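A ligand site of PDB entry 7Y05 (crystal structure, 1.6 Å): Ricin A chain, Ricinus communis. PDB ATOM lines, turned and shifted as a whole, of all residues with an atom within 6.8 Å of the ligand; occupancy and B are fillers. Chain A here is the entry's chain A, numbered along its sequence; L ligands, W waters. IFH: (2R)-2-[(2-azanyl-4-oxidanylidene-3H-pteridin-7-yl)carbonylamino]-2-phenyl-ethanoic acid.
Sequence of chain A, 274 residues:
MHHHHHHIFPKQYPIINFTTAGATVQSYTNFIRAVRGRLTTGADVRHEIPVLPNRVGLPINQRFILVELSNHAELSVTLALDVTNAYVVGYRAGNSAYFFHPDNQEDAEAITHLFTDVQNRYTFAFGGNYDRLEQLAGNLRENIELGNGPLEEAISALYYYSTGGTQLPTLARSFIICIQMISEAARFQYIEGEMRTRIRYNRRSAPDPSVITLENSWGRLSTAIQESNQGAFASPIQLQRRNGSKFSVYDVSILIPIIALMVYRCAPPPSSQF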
ATOM      1  N   LEU A  81      20.835   5.557  17.971  1.00  0.00           N
ATOM      2  CA  LEU A  81      21.295   4.431  18.779  1.00  0.00           C
ATOM      3  C   LEU A  81      22.367   4.847  19.778  1.00  0.00           C
ATOM      4  O   LEU A  81      23.304   5.565  19.434  1.00  0.00           O
ATOM      5  CB  LEU A  81      21.792   3.259  17.901  1.00  0.00           C
ATOM      6  CG  LEU A  81      20.769   2.291  17.279  1.00  0.00           C
ATOM      7  CD1 LEU A  81      19.884   2.950  16.238  1.00  0.00           C
ATOM      8  CD2 LEU A  81      21.493   1.098  16.674  1.00  0.00           C
ATOM      9  N   ASN A  85      25.024   0.390  24.320  1.00  0.00           N
ATOM     10  CA  ASN A  85      24.161  -0.792  24.381  1.00  0.00           C
ATOM     11  C   ASN A  85      23.402  -1.120  23.098  1.00  0.00           C
ATOM     12  O   ASN A  85      22.639  -2.081  23.061  1.00  0.00           O
ATOM     13  CB  ASN A  85      23.190  -0.690  25.575  1.00  0.00           C
ATOM     14  CG  ASN A  85      22.375   0.592  25.564  1.00  0.00           C
ATOM     15  OD1 ASN A  85      22.222   1.248  24.527  1.00  0.00           O
ATOM     16  ND2 ASN A  85      21.843   0.950  26.727  1.00  0.00           N
ATOM     17  N   ALA A  86      23.649  -0.321  22.059  1.00  0.00           N
ATOM     18  CA  ALA A  86      22.937  -0.384  20.765  1.00  0.00           C
ATOM     19  C   ALA A  86      21.411  -0.138  20.845  1.00  0.00           C
ATOM     20  O   ALA A  86      20.700  -0.418  19.888  1.00  0.00           O
ATOM     21  CB  ALA A  86      23.260  -1.694  20.016  1.00  0.00           C
ATOM     22  N   TYR A  87      20.937   0.394  21.975  1.00  0.00           N
ATOM     23  CA  TYR A  87      19.502   0.698  22.147  1.00  0.00           C
ATOM     24  C   TYR A  87      19.050   1.826  21.239  1.00  0.00           C
ATOM     25  O   TYR A  87      19.754   2.824  21.075  1.00  0.00           O
ATOM     26  CB  TYR A  87      19.168   1.021  23.621  1.00  0.00           C
ATOM     27  CG  TYR A  87      18.796  -0.203  24.452  1.00  0.00           C
ATOM     28  CD1 TYR A  87      19.705  -1.240  24.643  1.00  0.00           C
ATOM     29  CD2 TYR A  87      17.540  -0.303  25.064  1.00  0.00           C
ATOM     30  CE1 TYR A  87      19.382  -2.368  25.388  1.00  0.00           C
ATOM     31  CE2 TYR A  87      17.210  -1.426  25.839  1.00  0.00           C
ATOM     32  CZ  TYR A  87      18.128  -2.453  25.982  1.00  0.00           C
ATOM     33  OH  TYR A  87      17.831  -3.572  26.725  1.00  0.00           O
ATOM     34  N   VAL A  88      17.889   1.639  20.622  1.00  0.00           N
ATOM     35  CA  VAL A  88      17.205   2.688  19.900  1.00  0.00           C
ATOM     36  C   VAL A  88      16.582   3.596  20.971  1.00  0.00           C
ATOM     37  O   VAL A  88      15.741   3.140  21.743  1.00  0.00           O
ATOM     38  CB  VAL A  88      16.118   2.130  18.956  1.00  0.00           C
ATOM     39  CG1 VAL A  88      15.375   3.261  18.256  1.00  0.00           C
ATOM     40  CG2 VAL A  88      16.727   1.178  17.937  1.00  0.00           C
ATOM     41  N   VAL A  89      17.045   4.834  21.029  1.00  0.00           N
ATOM     42  CA  VAL A  89      16.574   5.773  22.065  1.00  0.00           C
ATOM     43  C   VAL A  89      15.484   6.711  21.562  1.00  0.00           C
ATOM     44  O   VAL A  89      14.779   7.341  22.360  1.00  0.00           O
ATOM     45  CB  VAL A  89      17.732   6.585  22.717  1.00  0.00           C
ATOM     46  CG1 VAL A  89      18.742   5.646  23.369  1.00  0.00           C
ATOM     47  CG2 VAL A  89      18.391   7.523  21.711  1.00  0.00           C
ATOM     48  N   GLY A  90      15.345   6.781  20.251  1.00  0.00           N
ATOM     49  CA  GLY A  90      14.327   7.627  19.632  1.00  0.00           C
ATOM     50  C   GLY A  90      14.487   7.698  18.133  1.00  0.00           C
ATOM     51  O   GLY A  90      15.365   7.047  17.560  1.00  0.00           O
ATOM     52  N   PHE A 100      12.073   7.621  23.650  1.00  0.00           N
ATOM     53  CA  PHE A 100      11.544   6.781  24.719  1.00  0.00           C
ATOM     54  C   PHE A 100      11.844   7.437  26.064  1.00  0.00           C
ATOM     55  O   PHE A 100      12.829   8.161  26.209  1.00  0.00           O
ATOM     56  CB  PHE A 100      12.122   5.360  24.655  1.00  0.00           C
ATOM     57  CG  PHE A 100      11.751   4.617  23.413  1.00  0.00           C
ATOM     58  CD1 PHE A 100      10.412   4.298  23.134  1.00  0.00           C
ATOM     59  CD2 PHE A 100      12.740   4.208  22.511  1.00  0.00           C
ATOM     60  CE1 PHE A 100      10.078   3.593  21.977  1.00  0.00           C
ATOM     61  CE2 PHE A 100      12.405   3.507  21.363  1.00  0.00           C
ATOM     62  CZ  PHE A 100      11.071   3.200  21.090  1.00  0.00           C
ATOM     63  N   GLY A 127       8.729   3.707  28.245  1.00  0.00           N
ATOM     64  CA  GLY A 127      10.084   3.260  27.890  1.00  0.00           C
ATOM     65  C   GLY A 127      10.070   2.379  26.654  1.00  0.00           C
ATOM     66  O   GLY A 127       9.019   1.946  26.198  1.00  0.00           O
ATOM     67  N   GLY A 128      11.266   2.119  26.131  1.00  0.00           N
ATOM     68  CA  GLY A 128      11.421   1.387  24.871  1.00  0.00           C
ATOM     69  C   GLY A 128      11.751  -0.089  24.969  1.00  0.00           C
ATOM     70  O   GLY A 128      12.124  -0.683  23.960  1.00  0.00           O
ATOM     71  N   ASN A 129      11.627  -0.673  26.160  1.00  0.00           N
ATOM     72  CA  ASN A 129      11.885  -2.104  26.374  1.00  0.00           C
ATOM     73  C   ASN A 129      10.797  -2.978  25.736  1.00  0.00           C
ATOM     74  O   ASN A 129       9.679  -2.523  25.517  1.00  0.00           O
ATOM     75  CB  ASN A 129      12.021  -2.407  27.863  1.00  0.00           C
ATOM     76  CG  ASN A 129      13.330  -1.925  28.450  1.00  0.00           C
ATOM     77  OD1 ASN A 129      14.149  -1.328  27.743  1.00  0.00           O
ATOM     78  ND2 ASN A 129      13.542  -2.176  29.731  1.00  0.00           N
ATOM     79  N   TYR A 130      11.154  -4.222  25.425  1.00  0.00           N
ATOM     80  CA  TYR A 130      10.218  -5.162  24.787  1.00  0.00           C
ATOM     81  C   TYR A 130       8.932  -5.376  25.584  1.00  0.00           C
ATOM     82  O   TYR A 130       7.851  -5.346  25.004  1.00  0.00           O
ATOM     83  CB  TYR A 130      10.855  -6.522  24.510  1.00  0.00           C
ATOM     84  CG  TYR A 130      11.905  -6.545  23.406  1.00  0.00           C
ATOM     85  CD1 TYR A 130      11.704  -5.889  22.188  1.00  0.00           C
ATOM     86  CD2 TYR A 130      13.091  -7.272  23.582  1.00  0.00           C
ATOM     87  CE1 TYR A 130      12.669  -5.929  21.186  1.00  0.00           C
ATOM     88  CE2 TYR A 130      14.055  -7.308  22.589  1.00  0.00           C
ATOM     89  CZ  TYR A 130      13.839  -6.642  21.399  1.00  0.00           C
ATOM     90  OH  TYR A 130      14.805  -6.706  20.430  1.00  0.00           O
ATOM     91  N   ASP A 131       9.079  -5.573  26.901  1.00  0.00           N
ATOM     92  CA  ASP A 131       7.928  -5.774  27.803  1.00  0.00           C
ATOM     93  C   ASP A 131       6.841  -4.710  27.596  1.00  0.00           C
ATOM     94  O   ASP A 131       5.668  -5.050  27.418  1.00  0.00           O
ATOM     95  CB  ASP A 131       8.377  -5.786  29.278  1.00  0.00           C
ATOM     96  CG  ASP A 131       8.859  -7.152  29.758  1.00  0.00           C
ATOM     97  OD1 ASP A 131       8.758  -8.148  29.003  1.00  0.00           O
ATOM     98  OD2 ASP A 131       9.340  -7.237  30.904  1.00  0.00           O
ATOM     99  N   LEU A 133       6.755  -2.412  24.971  1.00  0.00           N
ATOM    100  CA  LEU A 133       6.373  -2.338  23.560  1.00  0.00           C
ATOM    101  C   LEU A 133       5.390  -3.432  23.136  1.00  0.00           C
ATOM    102  O   LEU A 133       4.475  -3.171  22.370  1.00  0.00           O
ATOM    103  CB  LEU A 133       7.605  -2.318  22.640  1.00  0.00           C
ATOM    104  CG  LEU A 133       8.507  -1.077  22.654  1.00  0.00           C
ATOM    105  CD1 LEU A 133       9.664  -1.289  21.695  1.00  0.00           C
ATOM    106  CD2 LEU A 133       7.784   0.229  22.306  1.00  0.00           C
ATOM    107  N   ARG A 141       6.644 -10.612  20.763  1.00  0.00           N
ATOM    108  CA  ARG A 141       7.627 -10.780  19.690  1.00  0.00           C
ATOM    109  C   ARG A 141       7.434 -12.079  18.883  1.00  0.00           C
ATOM    110  O   ARG A 141       7.614 -12.076  17.663  1.00  0.00           O
ATOM    111  CB  ARG A 141       9.047 -10.733  20.261  1.00  0.00           C
ATOM    112  CG  ARG A 141       9.585  -9.340  20.496  1.00  0.00           C
ATOM    113  CD  ARG A 141      10.861  -9.408  21.321  1.00  0.00           C
ATOM    114  NE  ARG A 141      10.596  -9.745  22.715  1.00  0.00           N
ATOM    115  CZ  ARG A 141      11.480 -10.290  23.558  1.00  0.00           C
ATOM    116  NH1 ARG A 141      12.707 -10.581  23.152  1.00  0.00           N
ATOM    117  NH2 ARG A 141      11.129 -10.536  24.814  1.00  0.00           N
ATOM    118  N   PHE A 175       8.450  -0.371  16.059  1.00  0.00           N
ATOM    119  CA  PHE A 175       9.660  -0.291  16.875  1.00  0.00           C
ATOM    120  C   PHE A 175      10.267  -1.676  17.107  1.00  0.00           C
ATOM    121  O   PHE A 175      11.483  -1.860  16.938  1.00  0.00           O
ATOM    122  CB  PHE A 175       9.397   0.375  18.235  1.00  0.00           C
ATOM    123  CG  PHE A 175       9.239   1.874  18.174  1.00  0.00           C
ATOM    124  CD1 PHE A 175      10.126   2.661  17.426  1.00  0.00           C
ATOM    125  CD2 PHE A 175       8.227   2.504  18.891  1.00  0.00           C
ATOM    126  CE1 PHE A 175       9.988   4.046  17.388  1.00  0.00           C
ATOM    127  CE2 PHE A 175       8.089   3.889  18.852  1.00  0.00           C
ATOM    128  CZ  PHE A 175       8.967   4.656  18.102  1.00  0.00           C
ATOM    129  N   ILE A 179      14.014  -2.579  16.031  1.00  0.00           N
ATOM    130  CA  ILE A 179      14.958  -2.961  17.079  1.00  0.00           C
ATOM    131  C   ILE A 179      15.595  -4.321  16.802  1.00  0.00           C
ATOM    132  O   ILE A 179      16.818  -4.473  16.918  1.00  0.00           O
ATOM    133  CB  ILE A 179      14.310  -2.914  18.482  1.00  0.00           C
ATOM    134  CG1 ILE A 179      14.000  -1.465  18.876  1.00  0.00           C
ATOM    135  CG2 ILE A 179      15.225  -3.553  19.527  1.00  0.00           C
ATOM    136  CD1 ILE A 179      12.904  -1.321  19.907  1.00  0.00           C
ATOM    137  N   GLN A 180      14.779  -5.293  16.433  1.00  0.00           N
ATOM    138  CA  GLN A 180      15.307  -6.631  16.170  1.00  0.00           C
ATOM    139  C   GLN A 180      16.155  -6.701  14.905  1.00  0.00           C
ATOM    140  O   GLN A 180      17.178  -7.385  14.893  1.00  0.00           O
ATOM    141  CB  GLN A 180      14.185  -7.650  16.131  1.00  0.00           C
ATOM    142  CG  GLN A 180      13.568  -7.875  17.499  1.00  0.00           C
ATOM    143  CD  GLN A 180      12.405  -8.837  17.419  1.00  0.00           C
ATOM    144  OE1 GLN A 180      11.282  -8.433  17.102  1.00  0.00           O
ATOM    145  NE2 GLN A 180      12.675 -10.100  17.666  1.00  0.00           N
ATOM    146  N   SER A 183      19.290  -3.405  15.921  1.00  0.00           N
ATOM    147  CA  SER A 183      20.054  -3.556  17.166  1.00  0.00           C
ATOM    148  C   SER A 183      20.390  -5.006  17.507  1.00  0.00           C
ATOM    149  O   SER A 183      21.539  -5.325  17.798  1.00  0.00           O
ATOM    150  CB  SER A 183      19.319  -2.878  18.327  1.00  0.00           C
ATOM    151  OG  SER A 183      19.134  -1.506  18.047  1.00  0.00           O
ATOM    152  N   GLU A 184      19.393  -5.900  17.442  1.00  0.00           N
ATOM    153  CA  GLU A 184      19.636  -7.312  17.768  1.00  0.00           C
ATOM    154  C   GLU A 184      20.540  -7.985  16.741  1.00  0.00           C
ATOM    155  O   GLU A 184      21.382  -8.810  17.103  1.00  0.00           O
ATOM    156  CB  GLU A 184      18.347  -8.115  17.969  1.00  0.00           C
ATOM    157  CG  GLU A 184      17.421  -7.584  19.040  1.00  0.00           C
ATOM    158  CD  GLU A 184      17.926  -7.720  20.479  1.00  0.00           C
ATOM    159  OE1 GLU A 184      19.101  -8.094  20.709  1.00  0.00           O
ATOM    160  OE2 GLU A 184      17.124  -7.422  21.383  1.00  0.00           O
ATOM    161  N   ARG A 187      24.031  -6.977  17.533  1.00  0.00           N
ATOM    162  CA  ARG A 187      24.506  -7.669  18.735  1.00  0.00           C
ATOM    163  C   ARG A 187      24.830  -9.140  18.485  1.00  0.00           C
ATOM    164  O   ARG A 187      25.759  -9.683  19.075  1.00  0.00           O
ATOM    165  CB  ARG A 187      23.461  -7.609  19.843  1.00  0.00           C
ATOM    166  CG  ARG A 187      23.262  -6.242  20.463  1.00  0.00           C
ATOM    167  CD  ARG A 187      22.021  -6.267  21.330  1.00  0.00           C
ATOM    168  NE  ARG A 187      21.676  -4.914  21.768  1.00  0.00           N
ATOM    169  CZ  ARG A 187      20.442  -4.415  21.807  1.00  0.00           C
ATOM    170  NH1 ARG A 187      19.400  -5.140  21.435  1.00  0.00           N
ATOM    171  NH2 ARG A 187      20.261  -3.179  22.203  1.00  0.00           N
ATOM    172  N   GLU A 215      17.873 -12.666  22.590  1.00  0.00           N
ATOM    173  CA  GLU A 215      17.528 -11.268  22.872  1.00  0.00           C
ATOM    174  C   GLU A 215      17.339 -11.036  24.368  1.00  0.00           C
ATOM    175  O   GLU A 215      17.882 -10.078  24.933  1.00  0.00           O
ATOM    176  CB  GLU A 215      16.265 -10.847  22.136  1.00  0.00           C
ATOM    177  CG  GLU A 215      16.366 -10.936  20.620  1.00  0.00           C
ATOM    178  CD  GLU A 215      15.060 -10.665  19.907  1.00  0.00           C
ATOM    179  OE1 GLU A 215      14.003 -10.574  20.577  1.00  0.00           O
ATOM    180  OE2 GLU A 215      15.094 -10.542  18.673  1.00  0.00           O
ATOM    181  N   ASN A 216      16.599 -11.942  25.018  1.00  0.00           N
ATOM    182  CA  ASN A 216      16.320 -11.841  26.458  1.00  0.00           C
ATOM    183  C   ASN A 216      17.555 -11.989  27.329  1.00  0.00           C
ATOM    184  O   ASN A 216      17.610 -11.430  28.422  1.00  0.00           O
ATOM    185  CB  ASN A 216      15.284 -12.887  26.884  1.00  0.00           C
ATOM    186  CG  ASN A 216      13.900 -12.629  26.293  1.00  0.00           C
ATOM    187  OD1 ASN A 216      13.591 -11.521  25.861  1.00  0.00           O
ATOM    188  ND2 ASN A 216      13.055 -13.654  26.313  1.00  0.00           N
ATOM    189  N   TRP A 218      20.854 -11.266  26.397  1.00  0.00           N
ATOM    190  CA  TRP A 218      22.051 -10.520  25.961  1.00  0.00           C
ATOM    191  C   TRP A 218      22.859  -9.926  27.121  1.00  0.00           C
ATOM    192  O   TRP A 218      24.080 -10.085  27.162  1.00  0.00           O
ATOM    193  CB  TRP A 218      21.692  -9.429  24.955  1.00  0.00           C
ATOM    194  CG  TRP A 218      22.899  -8.694  24.392  1.00  0.00           C
ATOM    195  CD1 TRP A 218      23.941  -9.242  23.705  1.00  0.00           C
ATOM    196  CD2 TRP A 218      23.176  -7.289  24.489  1.00  0.00           C
ATOM    197  NE1 TRP A 218      24.853  -8.263  23.356  1.00  0.00           N
ATOM    198  CE2 TRP A 218      24.406  -7.059  23.824  1.00  0.00           C
ATOM    199  CE3 TRP A 218      22.497  -6.208  25.073  1.00  0.00           C
ATOM    200  CZ2 TRP A 218      24.969  -5.769  23.709  1.00  0.00           C
ATOM    201  CZ3 TRP A 218      23.056  -4.925  24.962  1.00  0.00           C
ATOM    202  CH2 TRP A 218      24.291  -4.716  24.285  1.00  0.00           C
HETATM  203  C7  IFH L   1      15.336  -4.603  24.669  1.00  0.00           C
HETATM  204  C6  IFH L   1      16.508  -4.920  23.950  1.00  0.00           C
HETATM  205  N1  IFH L   1      14.598  -1.374  23.358  1.00  0.00           N
HETATM  206  C2  IFH L   1      15.017  -0.446  22.483  1.00  0.00           C
HETATM  207  N2  IFH L   1      14.336   0.680  22.357  1.00  0.00           N
HETATM  208  N3  IFH L   1      16.175  -0.675  21.720  1.00  0.00           N
HETATM  209  C4  IFH L   1      16.879  -1.875  21.883  1.00  0.00           C
HETATM  210  N   IFH L   1      15.489  -6.594  25.898  1.00  0.00           N
HETATM  211  CAM IFH L   1      14.789  -5.474  25.640  1.00  0.00           C
HETATM  212  OAO IFH L   1      13.765  -5.180  26.250  1.00  0.00           O
HETATM  213  N8  IFH L   1      14.742  -3.414  24.432  1.00  0.00           N
HETATM  214  C8A IFH L   1      15.234  -2.540  23.533  1.00  0.00           C
HETATM  215  O4  IFH L   1      17.882  -2.064  21.199  1.00  0.00           O
HETATM  216  C4A IFH L   1      16.402  -2.821  22.807  1.00  0.00           C
HETATM  217  N5  IFH L   1      17.022  -4.003  23.010  1.00  0.00           N
HETATM  218  O   HOH W   1      11.689  -5.890  28.264  1.00  0.00           O
HETATM  219  O   HOH W   2      18.971  -6.095  26.010  1.00  0.00           O
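Water W1 lies within hydrogen-bond range of the backbone NH (N) of Asp 131 (3.0 Å), an oxygen (OAO) of the ligand (3.0 Å) and the backbone NH (N) of Tyr 130 (3.3 Å).
OG of Ser 183 sits at hydrogen-bond distance from O of Ala 86, at 2.7 Å.
N of Glu 184 lies within hydrogen-bond range of O of Ile 179 (3.0 Å).
OE2 of Glu 184 is in hydrogen-bond range of OH of Tyr 130 (2.6 Å).
N of Phe 100 lies within hydrogen-bond range of O of Val 89.
The backbone carbonyl oxygen (O) of Asn 85 is in hydrogen-bond range of the guanidinium group (NH2) of Arg 187 (2.8 Å).
The guanidinium group (NH1) of Arg 187 lies within salt-bridge range of the side-chain carboxylate (OE1) of Glu 184 (3.1 Å).
The backbone NH of Tyr 87 sits at hydrogen-bond distance from the side-chain amide oxygen of Asn 85 (3.0 Å).
A nitrogen (N2) of the ligand sits at hydrogen-bond distance from the backbone carbonyl oxygen (O) of Gly 128.
The guanidinium group (NH2) of Arg 187 sits at hydrogen-bond distance from an oxygen (O4) of the ligand, 2.8 Å away.
N of Tyr 130 is in hydrogen-bond range of OAO of the ligand, 2.9 Å away.
O4 of the ligand lies close to OG of Ser 183 (3.4 Å).
The backbone carbonyl oxygen of Val 88 lies within hydrogen-bond range of a nitrogen (N2) of the ligand (2.9 Å).
Residues that only touch the ligand: Ala 86 (3.5 Å), Tyr 87 (3.2 Å), Phe 100 (3.6 Å), Asn 129 (3.6 Å), Ile 179 (3.3 Å) and Glu 184 (3.6 Å).
Hydrophobic or aromatic side chains that line the ligand: Tyr 87, Val 88, Phe 100, Tyr 130 and Ile 179.
Of the 24 residues printed, 11 come within 4 Å of the ligand.
The nearest printed residue that does not touch the ligand is Glu 215 (4.3 Å).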
